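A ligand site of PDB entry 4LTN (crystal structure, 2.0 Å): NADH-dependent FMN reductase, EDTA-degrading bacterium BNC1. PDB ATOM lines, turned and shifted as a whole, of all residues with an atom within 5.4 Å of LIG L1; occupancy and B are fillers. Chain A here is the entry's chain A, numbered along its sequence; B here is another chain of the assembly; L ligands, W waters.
O4 of LIG L1 lies within hydrogen-bond range of O1 of LG2 L2 (2.8 Å).
The side-chain hydroxyl (OG1) of Thr 18 is in hydrogen-bond range of the side-chain hydroxyl (OG1) of Thr 110, 3.0 Å away. The side-chain amino group (NZ) of Lys 81 sits at hydrogen-bond distance from the backbone carbonyl oxygen (O) of Leu 95 of chain B (2.9 Å). OG of Ser 11 lies within hydrogen-bond range of N of Ser 13, at 3.0 Å. O of Gly 111 is in hydrogen-bond range of N of Gln 144, 2.7 Å away. The side-chain hydroxyl of Ser 16 lies within hydrogen-bond range of the backbone NH of Ala 19 (2.9 Å). The backbone carbonyl oxygen of Lys 81 lies close to the side-chain hydroxyl of Ser 130 of chain B, 3.5 Å away. The side-chain amide nitrogen (NE2) of Gln 144 sits at hydrogen-bond distance from the side-chain hydroxyl (OG1) of Thr 17, 3.3 Å away. The backbone NH (N) of Thr 18 lies close to the side-chain hydroxyl (OG) of Ser 16, at 3.2 Å.
Ser 13 touches LIG L1. CB of Pro 78 touches O6 of LIG L1 (3.4 Å). CA of Tyr 80 touches N3 of LIG L1, 3.4 Å away. Gly 111 touches LIG L1 (CA to O3, 3.4 Å). Asp 93 of chain B touches LIG L1. Hydrophobic or aromatic side chains that line LIG L1: Pro 78, Ile 79, Tyr 80 and His 116. 17 residues have an atom within 4 Å of LIG L1: Ser 11, Ser 13, Ser 16, Thr 17, Thr 18, Pro 78, Ile 79, Tyr 80, Lys 81, Ala 82, Thr 110, Gly 111, Gly 112, Ser 113, His 116, Gln 144 and Asp 93 of chain B. The nearest printed residue that does not touch LIG L1 is Asn 15 (4.1 Å).
Water W3 lies within hydrogen-bond range of an oxygen (O8) of LIG L1 (2.6 Å) and the side-chain hydroxyl (OH) of Tyr 80 (2.7 Å).
O3 of LIG L1 sits at hydrogen-bond distance from N of Ile 79, at 3.4 Å. N4 of LG2 L2 is in hydrogen-bond range of NZ of Lys 81 (3.3 Å). An oxygen (O9) of LIG L1 lies within hydrogen-bond range of the side-chain hydroxyl of Ser 16, 2.4 Å away. A ring nitrogen (ND1) of His 116 sits at hydrogen-bond distance from a nitrogen (N2) of LIG L1. The backbone NH (N) of Thr 17 lies within hydrogen-bond range of an oxygen (O7) of LIG L1 (2.9 Å). O3 of LIG L1 is in hydrogen-bond range of O of Ile 79 (2.7 Å). The side-chain amide oxygen (OE1) of Gln 144 lies within hydrogen-bond range of an oxygen (O5) of LIG L1 (2.5 Å). An oxygen (O8) of LIG L1 is in hydrogen-bond range of the side-chain hydroxyl (OG) of Ser 11, at 2.4 Å. N of Gly 112 is in hydrogen-bond range of N1 of LIG L1. The side-chain hydroxyl of Thr 110 lies within hydrogen-bond range of an oxygen (O5) of LIG L1. An oxygen (O9) of LIG L1 lies within hydrogen-bond range of the side-chain hydroxyl (OG1) of Thr 18. The backbone NH of Lys 81 lies within hydrogen-bond range of a nitrogen (N3) of LIG L1, 3.1 Å away. N of Ala 82 sits at hydrogen-bond distance from O2 of LIG L1, 2.9 Å away. O1 of LIG L1 sits at hydrogen-bond distance from N of Ser 113, 3.1 Å away. N of Thr 18 is in hydrogen-bond range of O9 of LIG L1 (2.9 Å).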
ATOM      1  N   SER A  11      20.275 -17.473 -20.213  1.00  0.00           N
ATOM      2  CA  SER A  11      19.720 -18.477 -19.331  1.00  0.00           C
ATOM      3  C   SER A  11      19.469 -19.755 -20.132  1.00  0.00           C
ATOM      4  O   SER A  11      18.997 -19.694 -21.258  1.00  0.00           O
ATOM      5  CB  SER A  11      18.430 -18.009 -18.682  1.00  0.00           C
ATOM      6  OG  SER A  11      17.856 -19.054 -17.903  1.00  0.00           O
ATOM      7  N   PRO A  12      19.811 -20.921 -19.559  1.00  0.00           N
ATOM      8  CA  PRO A  12      19.480 -22.181 -20.229  1.00  0.00           C
ATOM      9  C   PRO A  12      18.064 -22.607 -19.877  1.00  0.00           C
ATOM     10  O   PRO A  12      17.606 -23.667 -20.269  1.00  0.00           O
ATOM     11  CB  PRO A  12      20.492 -23.165 -19.620  1.00  0.00           C
ATOM     12  CG  PRO A  12      20.725 -22.626 -18.220  1.00  0.00           C
ATOM     13  CD  PRO A  12      20.579 -21.117 -18.313  1.00  0.00           C
ATOM     14  N   SER A  13      17.361 -21.758 -19.129  1.00  0.00           N
ATOM     15  CA  SER A  13      16.041 -22.122 -18.654  1.00  0.00           C
ATOM     16  C   SER A  13      14.958 -21.568 -19.570  1.00  0.00           C
ATOM     17  O   SER A  13      15.081 -20.470 -20.097  1.00  0.00           O
ATOM     18  CB  SER A  13      15.848 -21.619 -17.225  1.00  0.00           C
ATOM     19  OG  SER A  13      14.501 -21.700 -16.823  1.00  0.00           O
ATOM     20  N   ASN A  15      11.305 -19.943 -20.296  1.00  0.00           N
ATOM     21  CA  ASN A  15      10.597 -18.906 -19.558  1.00  0.00           C
ATOM     22  C   ASN A  15      11.556 -18.090 -18.674  1.00  0.00           C
ATOM     23  O   ASN A  15      11.342 -17.928 -17.472  1.00  0.00           O
ATOM     24  CB  ASN A  15       9.489 -19.526 -18.710  1.00  0.00           C
ATOM     25  CG  ASN A  15       8.524 -18.492 -18.184  1.00  0.00           C
ATOM     26  OD1 ASN A  15       8.290 -17.467 -18.831  1.00  0.00           O
ATOM     27  ND2 ASN A  15       7.975 -18.733 -16.996  1.00  0.00           N
ATOM     28  N   SER A  16      12.610 -17.572 -19.291  1.00  0.00           N
ATOM     29  CA  SER A  16      13.671 -16.846 -18.591  1.00  0.00           C
ATOM     30  C   SER A  16      13.255 -15.446 -18.143  1.00  0.00           C
ATOM     31  O   SER A  16      12.888 -14.607 -18.969  1.00  0.00           O
ATOM     32  CB  SER A  16      14.877 -16.747 -19.539  1.00  0.00           C
ATOM     33  OG  SER A  16      15.919 -15.937 -19.016  1.00  0.00           O
ATOM     34  N   THR A  17      13.346 -15.173 -16.852  1.00  0.00           N
ATOM     35  CA  THR A  17      13.191 -13.810 -16.344  1.00  0.00           C
ATOM     36  C   THR A  17      14.295 -12.912 -16.886  1.00  0.00           C
ATOM     37  O   THR A  17      14.071 -11.743 -17.214  1.00  0.00           O
ATOM     38  CB  THR A  17      13.225 -13.776 -14.810  1.00  0.00           C
ATOM     39  OG1 THR A  17      12.108 -14.499 -14.291  1.00  0.00           O
ATOM     40  CG2 THR A  17      13.154 -12.335 -14.294  1.00  0.00           C
ATOM     41  N   THR A  18      15.502 -13.455 -16.983  1.00  0.00           N
ATOM     42  CA  THR A  18      16.632 -12.716 -17.527  1.00  0.00           C
ATOM     43  C   THR A  18      16.369 -12.264 -18.963  1.00  0.00           C
ATOM     44  O   THR A  18      16.716 -11.152 -19.358  1.00  0.00           O
ATOM     45  CB  THR A  18      17.919 -13.581 -17.519  1.00  0.00           C
ATOM     46  OG1 THR A  18      18.135 -14.109 -16.210  1.00  0.00           O
ATOM     47  CG2 THR A  18      19.127 -12.748 -17.927  1.00  0.00           C
ATOM     48  N   ALA A  19      15.752 -13.142 -19.754  1.00  0.00           N
ATOM     49  CA  ALA A  19      15.403 -12.790 -21.140  1.00  0.00           C
ATOM     50  C   ALA A  19      14.381 -11.651 -21.164  1.00  0.00           C
ATOM     51  O   ALA A  19      14.432 -10.764 -22.008  1.00  0.00           O
ATOM     52  CB  ALA A  19      14.842 -14.020 -21.887  1.00  0.00           C
ATOM     53  N   PRO A  78      21.464 -14.951 -16.004  1.00  0.00           N
ATOM     54  CA  PRO A  78      21.149 -15.238 -14.603  1.00  0.00           C
ATOM     55  C   PRO A  78      22.468 -15.520 -13.897  1.00  0.00           C
ATOM     56  O   PRO A  78      23.465 -15.836 -14.559  1.00  0.00           O
ATOM     57  CB  PRO A  78      20.335 -16.533 -14.694  1.00  0.00           C
ATOM     58  CG  PRO A  78      20.829 -17.169 -15.900  1.00  0.00           C
ATOM     59  CD  PRO A  78      21.104 -16.078 -16.880  1.00  0.00           C
ATOM     60  N   ILE A  79      22.496 -15.390 -12.579  1.00  0.00           N
ATOM     61  CA  ILE A  79      23.679 -15.782 -11.842  1.00  0.00           C
ATOM     62  C   ILE A  79      23.614 -17.280 -11.555  1.00  0.00           C
ATOM     63  O   ILE A  79      22.683 -17.754 -10.924  1.00  0.00           O
ATOM     64  CB  ILE A  79      23.819 -14.991 -10.518  1.00  0.00           C
ATOM     65  CG1 ILE A  79      23.929 -13.479 -10.802  1.00  0.00           C
ATOM     66  CG2 ILE A  79      25.015 -15.482  -9.740  1.00  0.00           C
ATOM     67  CD1 ILE A  79      24.981 -13.104 -11.870  1.00  0.00           C
ATOM     68  N   TYR A  80      24.611 -18.016 -12.069  1.00  0.00           N
ATOM     69  CA  TYR A  80      24.753 -19.452 -11.811  1.00  0.00           C
ATOM     70  C   TYR A  80      26.108 -19.669 -11.130  1.00  0.00           C
ATOM     71  O   TYR A  80      27.147 -19.291 -11.678  1.00  0.00           O
ATOM     72  CB  TYR A  80      24.753 -20.242 -13.138  1.00  0.00           C
ATOM     73  CG  TYR A  80      23.396 -20.658 -13.678  1.00  0.00           C
ATOM     74  CD1 TYR A  80      22.226 -19.996 -13.317  1.00  0.00           C
ATOM     75  CD2 TYR A  80      23.277 -21.738 -14.560  1.00  0.00           C
ATOM     76  CE1 TYR A  80      20.989 -20.374 -13.820  1.00  0.00           C
ATOM     77  CE2 TYR A  80      22.037 -22.136 -15.073  1.00  0.00           C
ATOM     78  CZ  TYR A  80      20.898 -21.453 -14.691  1.00  0.00           C
ATOM     79  OH  TYR A  80      19.661 -21.807 -15.170  1.00  0.00           O
ATOM     80  N   LYS A  81      26.106 -20.304  -9.958  1.00  0.00           N
ATOM     81  CA  LYS A  81      27.363 -20.601  -9.257  1.00  0.00           C
ATOM     82  C   LYS A  81      28.202 -19.329  -9.099  1.00  0.00           C
ATOM     83  O   LYS A  81      29.397 -19.332  -9.361  1.00  0.00           O
ATOM     84  CB  LYS A  81      28.182 -21.659 -10.018  1.00  0.00           C
ATOM     85  CG  LYS A  81      27.778 -23.123  -9.721  1.00  0.00           C
ATOM     86  CD  LYS A  81      26.300 -23.339  -9.923  1.00  0.00           C
ATOM     87  CE  LYS A  81      25.962 -24.831 -10.080  1.00  0.00           C
ATOM     88  NZ  LYS A  81      25.980 -25.542  -8.784  1.00  0.00           N
ATOM     89  N   ALA A  82      27.555 -18.230  -8.713  1.00  0.00           N
ATOM     90  CA  ALA A  82      28.244 -16.968  -8.411  1.00  0.00           C
ATOM     91  C   ALA A  82      28.925 -16.318  -9.607  1.00  0.00           C
ATOM     92  O   ALA A  82      29.885 -15.573  -9.434  1.00  0.00           O
ATOM     93  CB  ALA A  82      29.260 -17.178  -7.273  1.00  0.00           C
ATOM     94  N   SER A  83      28.456 -16.625 -10.827  1.00  0.00           N
ATOM     95  CA  SER A  83      29.001 -15.979 -12.004  1.00  0.00           C
ATOM     96  C   SER A  83      27.998 -16.033 -13.171  1.00  0.00           C
ATOM     97  O   SER A  83      26.836 -16.419 -12.984  1.00  0.00           O
ATOM     98  CB  SER A  83      30.328 -16.642 -12.408  1.00  0.00           C
ATOM     99  OG  SER A  83      31.031 -15.868 -13.367  1.00  0.00           O
ATOM    100  N   THR A 110      19.899 -11.333 -13.328  1.00  0.00           N
ATOM    101  CA  THR A 110      18.963 -11.636 -12.269  1.00  0.00           C
ATOM    102  C   THR A 110      19.575 -12.757 -11.441  1.00  0.00           C
ATOM    103  O   THR A 110      20.363 -13.554 -11.955  1.00  0.00           O
ATOM    104  CB  THR A 110      17.571 -12.056 -12.813  1.00  0.00           C
ATOM    105  OG1 THR A 110      17.631 -13.369 -13.369  1.00  0.00           O
ATOM    106  CG2 THR A 110      17.139 -11.100 -13.913  1.00  0.00           C
ATOM    107  N   GLY A 111      19.228 -12.813 -10.168  1.00  0.00           N
ATOM    108  CA  GLY A 111      19.709 -13.888  -9.311  1.00  0.00           C
ATOM    109  C   GLY A 111      18.693 -14.186  -8.236  1.00  0.00           C
ATOM    110  O   GLY A 111      17.737 -13.427  -8.053  1.00  0.00           O
ATOM    111  N   GLY A 112      18.895 -15.286  -7.523  1.00  0.00           N
ATOM    112  CA  GLY A 112      17.982 -15.681  -6.468  1.00  0.00           C
ATOM    113  C   GLY A 112      18.234 -14.905  -5.189  1.00  0.00           C
ATOM    114  O   GLY A 112      17.359 -14.799  -4.340  1.00  0.00           O
ATOM    115  N   SER A 113      19.447 -14.368  -5.061  1.00  0.00           N
ATOM    116  CA  SER A 113      19.891 -13.729  -3.824  1.00  0.00           C
ATOM    117  C   SER A 113      20.638 -12.420  -4.093  1.00  0.00           C
ATOM    118  O   SER A 113      21.447 -12.336  -5.020  1.00  0.00           O
ATOM    119  CB  SER A 113      20.822 -14.671  -3.061  1.00  0.00           C
ATOM    120  OG  SER A 113      21.588 -13.962  -2.112  1.00  0.00           O
ATOM    121  N   HIS A 116      24.822 -11.981  -4.559  1.00  0.00           N
ATOM    122  CA  HIS A 116      25.708 -12.134  -5.711  1.00  0.00           C
ATOM    123  C   HIS A 116      25.709 -10.990  -6.715  1.00  0.00           C
ATOM    124  O   HIS A 116      26.118 -11.156  -7.873  1.00  0.00           O
ATOM    125  CB  HIS A 116      25.478 -13.492  -6.401  1.00  0.00           C
ATOM    126  CG  HIS A 116      25.975 -14.644  -5.604  1.00  0.00           C
ATOM    127  ND1 HIS A 116      25.611 -15.940  -5.843  1.00  0.00           N
ATOM    128  CD2 HIS A 116      26.806 -14.680  -4.528  1.00  0.00           C
ATOM    129  CE1 HIS A 116      26.202 -16.742  -4.972  1.00  0.00           C
ATOM    130  NE2 HIS A 116      26.939 -16.000  -4.160  1.00  0.00           N
ATOM    131  N   PHE A 141      21.650  -5.479 -11.503  1.00  0.00           N
ATOM    132  CA  PHE A 141      21.297  -6.815 -11.024  1.00  0.00           C
ATOM    133  C   PHE A 141      19.921  -6.742 -10.364  1.00  0.00           C
ATOM    134  O   PHE A 141      19.655  -5.861  -9.539  1.00  0.00           O
ATOM    135  CB  PHE A 141      22.339  -7.270 -10.006  1.00  0.00           C
ATOM    136  CG  PHE A 141      22.036  -8.594  -9.354  1.00  0.00           C
ATOM    137  CD1 PHE A 141      21.117  -8.681  -8.317  1.00  0.00           C
ATOM    138  CD2 PHE A 141      22.713  -9.739  -9.746  1.00  0.00           C
ATOM    139  CE1 PHE A 141      20.852  -9.890  -7.710  1.00  0.00           C
ATOM    140  CE2 PHE A 141      22.448 -10.948  -9.140  1.00  0.00           C
ATOM    141  CZ  PHE A 141      21.519 -11.037  -8.125  1.00  0.00           C
ATOM    142  N   GLN A 144      15.317 -12.192  -8.233  1.00  0.00           N
ATOM    143  CA  GLN A 144      14.230 -12.859  -8.973  1.00  0.00           C
ATOM    144  C   GLN A 144      12.847 -12.359  -8.574  1.00  0.00           C
ATOM    145  O   GLN A 144      12.021 -12.042  -9.432  1.00  0.00           O
ATOM    146  CB  GLN A 144      14.311 -14.381  -8.762  1.00  0.00           C
ATOM    147  CG  GLN A 144      13.324 -15.195  -9.614  1.00  0.00           C
ATOM    148  CD  GLN A 144      13.715 -15.217 -11.089  1.00  0.00           C
ATOM    149  OE1 GLN A 144      14.323 -14.274 -11.589  1.00  0.00           O
ATOM    150  NE2 GLN A 144      13.373 -16.316 -11.786  1.00  0.00           N
ATOM    151  N   ASP B  93      27.763 -25.845 -13.999  1.00  0.00           N
ATOM    152  CA  ASP B  93      26.416 -25.316 -13.793  1.00  0.00           C
ATOM    153  C   ASP B  93      25.403 -26.412 -13.476  1.00  0.00           C
ATOM    154  O   ASP B  93      24.423 -26.167 -12.786  1.00  0.00           O
ATOM    155  CB  ASP B  93      25.947 -24.523 -15.020  1.00  0.00           C
ATOM    156  CG  ASP B  93      26.595 -23.138 -15.108  1.00  0.00           C
ATOM    157  OD1 ASP B  93      27.197 -22.679 -14.098  1.00  0.00           O
ATOM    158  OD2 ASP B  93      26.501 -22.517 -16.201  1.00  0.00           O
ATOM    159  N   LEU B  95      25.970 -29.225 -11.699  1.00  0.00           N
ATOM    160  CA  LEU B  95      26.165 -29.859 -10.397  1.00  0.00           C
ATOM    161  C   LEU B  95      25.211 -29.282  -9.367  1.00  0.00           C
ATOM    162  O   LEU B  95      24.781 -28.140  -9.497  1.00  0.00           O
ATOM    163  CB  LEU B  95      27.615 -29.683  -9.902  1.00  0.00           C
ATOM    164  CG  LEU B  95      28.695 -30.113 -10.914  1.00  0.00           C
ATOM    165  CD1 LEU B  95      30.105 -29.814 -10.404  1.00  0.00           C
ATOM    166  CD2 LEU B  95      28.544 -31.600 -11.281  1.00  0.00           C
ATOM    167  N   SER B 130      31.510 -21.216  -4.343  1.00  0.00           N
ATOM    168  CA  SER B 130      30.043 -21.124  -4.310  1.00  0.00           C
ATOM    169  C   SER B 130      29.436 -22.512  -4.105  1.00  0.00           C
ATOM    170  O   SER B 130      28.264 -22.625  -3.760  1.00  0.00           O
ATOM    171  CB  SER B 130      29.495 -20.459  -5.575  1.00  0.00           C
ATOM    172  OG  SER B 130      29.259 -21.405  -6.603  1.00  0.00           O
HETATM  173  N1  LIG L   1      21.182 -17.292  -7.818  1.00  0.00           N
HETATM  174  C1  LIG L   1      22.147 -16.575  -7.137  1.00  0.00           C
HETATM  175  O1  LIG L   1      21.852 -15.503  -6.621  1.00  0.00           O
HETATM  176  N2  LIG L   1      23.436 -17.066  -7.030  1.00  0.00           N
HETATM  177  C2  LIG L   1      23.777 -18.283  -7.592  1.00  0.00           C
HETATM  178  O2  LIG L   1      24.932 -18.717  -7.496  1.00  0.00           O
HETATM  179  C3  LIG L   1      22.825 -19.004  -8.278  1.00  0.00           C
HETATM  180  N3  LIG L   1      23.156 -20.209  -8.859  1.00  0.00           N
HETATM  181  C4  LIG L   1      22.191 -20.915  -9.550  1.00  0.00           C
HETATM  182  C5  LIG L   1      22.519 -22.140 -10.142  1.00  0.00           C
HETATM  183  C6  LIG L   1      21.550 -22.863 -10.830  1.00  0.00           C
HETATM  184  C7  LIG L   1      21.894 -24.176 -11.471  1.00  0.00           C
HETATM  185  C8  LIG L   1      20.258 -22.359 -10.933  1.00  0.00           C
HETATM  186  C9  LIG L   1      19.216 -23.143 -11.682  1.00  0.00           C
HETATM  187  C10 LIG L   1      19.919 -21.133 -10.351  1.00  0.00           C
HETATM  188  C11 LIG L   1      20.889 -20.410  -9.663  1.00  0.00           C
HETATM  189  N4  LIG L   1      20.573 -19.189  -9.076  1.00  0.00           N
HETATM  190  C12 LIG L   1      21.530 -18.505  -8.388  1.00  0.00           C
HETATM  191  C13 LIG L   1      19.201 -18.612  -9.165  1.00  0.00           C
HETATM  192  C14 LIG L   1      19.031 -17.903 -10.511  1.00  0.00           C
HETATM  193  O3  LIG L   1      20.061 -16.956 -10.709  1.00  0.00           O
HETATM  194  C15 LIG L   1      17.694 -17.158 -10.570  1.00  0.00           C
HETATM  195  O4  LIG L   1      16.651 -18.104 -10.412  1.00  0.00           O
HETATM  196  C16 LIG L   1      17.527 -16.406 -11.883  1.00  0.00           C
HETATM  197  O5  LIG L   1      16.587 -15.367 -11.738  1.00  0.00           O
HETATM  198  C17 LIG L   1      17.112 -17.319 -13.026  1.00  0.00           C
HETATM  199  O6  LIG L   1      16.938 -16.547 -14.197  1.00  0.00           O
HETATM  200  P1  LIG L   1      16.197 -17.121 -15.515  1.00  0.00           P
HETATM  201  O7  LIG L   1      14.713 -17.150 -15.241  1.00  0.00           O
HETATM  202  O8  LIG L   1      16.729 -18.493 -15.835  1.00  0.00           O
HETATM  203  O9  LIG L   1      16.450 -16.203 -16.683  1.00  0.00           O
HETATM  204  P1  LG2 L   2      16.262 -19.075  -6.572  1.00  0.00           P
HETATM  205  O1  LG2 L   2      15.891 -18.170  -7.695  1.00  0.00           O
HETATM  206  O2  LG2 L   2      17.516 -18.687  -5.857  1.00  0.00           O
HETATM  207  O3  LG2 L   2      16.499 -20.549  -7.013  1.00  0.00           O
HETATM  208  C1  LG2 L   2      15.854 -21.057  -8.163  1.00  0.00           C
HETATM  209  C2  LG2 L   2      16.126 -22.493  -8.291  1.00  0.00           C
HETATM  210  O4  LG2 L   2      17.489 -22.758  -8.612  1.00  0.00           O
HETATM  211  C3  LG2 L   2      15.821 -23.227  -7.065  1.00  0.00           C
HETATM  212  O5  LG2 L   2      15.149 -24.369  -7.386  1.00  0.00           O
HETATM  213  C4  LG2 L   2      17.119 -23.569  -6.471  1.00  0.00           C
HETATM  214  O6  LG2 L   2      17.079 -24.848  -5.918  1.00  0.00           O
HETATM  215  C5  LG2 L   2      18.054 -23.573  -7.602  1.00  0.00           C
HETATM  216  N1  LG2 L   2      19.262 -23.075  -7.229  1.00  0.00           N
HETATM  217  C6  LG2 L   2      19.528 -21.997  -6.553  1.00  0.00           C
HETATM  218  N2  LG2 L   2      20.852 -21.889  -6.420  1.00  0.00           N
HETATM  219  C7  LG2 L   2      21.453 -22.923  -7.042  1.00  0.00           C
HETATM  220  C8  LG2 L   2      22.778 -23.341  -7.234  1.00  0.00           C
HETATM  221  N3  LG2 L   2      23.845 -22.583  -6.725  1.00  0.00           N
HETATM  222  N4  LG2 L   2      22.992 -24.443  -7.931  1.00  0.00           N
HETATM  223  C9  LG2 L   2      21.981 -25.131  -8.391  1.00  0.00           C
HETATM  224  N5  LG2 L   2      20.717 -24.798  -8.235  1.00  0.00           N
HETATM  225  C10 LG2 L   2      20.407 -23.696  -7.566  1.00  0.00           C
HETATM  226  O7  LG2 L   2      15.052 -19.027  -5.595  1.00  0.00           O
HETATM  227  P2  LG2 L   2      15.104 -19.279  -4.011  1.00  0.00           P
HETATM  228  O8  LG2 L   2      16.292 -20.138  -3.754  1.00  0.00           O
HETATM  229  O9  LG2 L   2      13.767 -19.914  -3.662  1.00  0.00           O
HETATM  230  O10 LG2 L   2      15.337 -17.854  -3.374  1.00  0.00           O
HETATM  231  C11 LG2 L   2      15.299 -17.489  -1.977  1.00  0.00           C
HETATM  232  C12 LG2 L   2      16.755 -17.280  -1.519  1.00  0.00           C
HETATM  233  O11 LG2 L   2      17.204 -15.954  -1.290  1.00  0.00           O
HETATM  234  C13 LG2 L   2      16.975 -17.915  -0.279  1.00  0.00           C
HETATM  235  O12 LG2 L   2      16.881 -19.317  -0.519  1.00  0.00           O
HETATM  236  C14 LG2 L   2      18.323 -17.463   0.045  1.00  0.00           C
HETATM  237  O13 LG2 L   2      19.250 -18.310  -0.562  1.00  0.00           O
HETATM  238  C15 LG2 L   2      18.446 -16.126  -0.592  1.00  0.00           C
HETATM  239  N6  LG2 L   2      18.631 -15.125   0.371  1.00  0.00           N
HETATM  240  C16 LG2 L   2      19.778 -14.427   0.494  1.00  0.00           C
HETATM  241  C17 LG2 L   2      19.907 -13.405   1.459  1.00  0.00           C
HETATM  242  C18 LG2 L   2      21.151 -12.510   1.651  1.00  0.00           C
HETATM  243  O14 LG2 L   2      21.004 -11.420   1.191  1.00  0.00           O
HETATM  244  N7  LG2 L   2      22.367 -12.848   2.342  1.00  0.00           N
HETATM  245  C19 LG2 L   2      18.803 -13.136   2.286  1.00  0.00           C
HETATM  246  C20 LG2 L   2      17.647 -13.881   2.136  1.00  0.00           C
HETATM  247  C21 LG2 L   2      17.610 -14.869   1.154  1.00  0.00           C
HETATM  248  O   HOH W   1      16.463 -20.406 -11.635  1.00  0.00           O
HETATM  249  O   HOH W   2      22.273 -27.489 -10.649  1.00  0.00           O
HETATM  250  O   HOH W   3      17.425 -20.561 -14.349  1.00  0.00           O
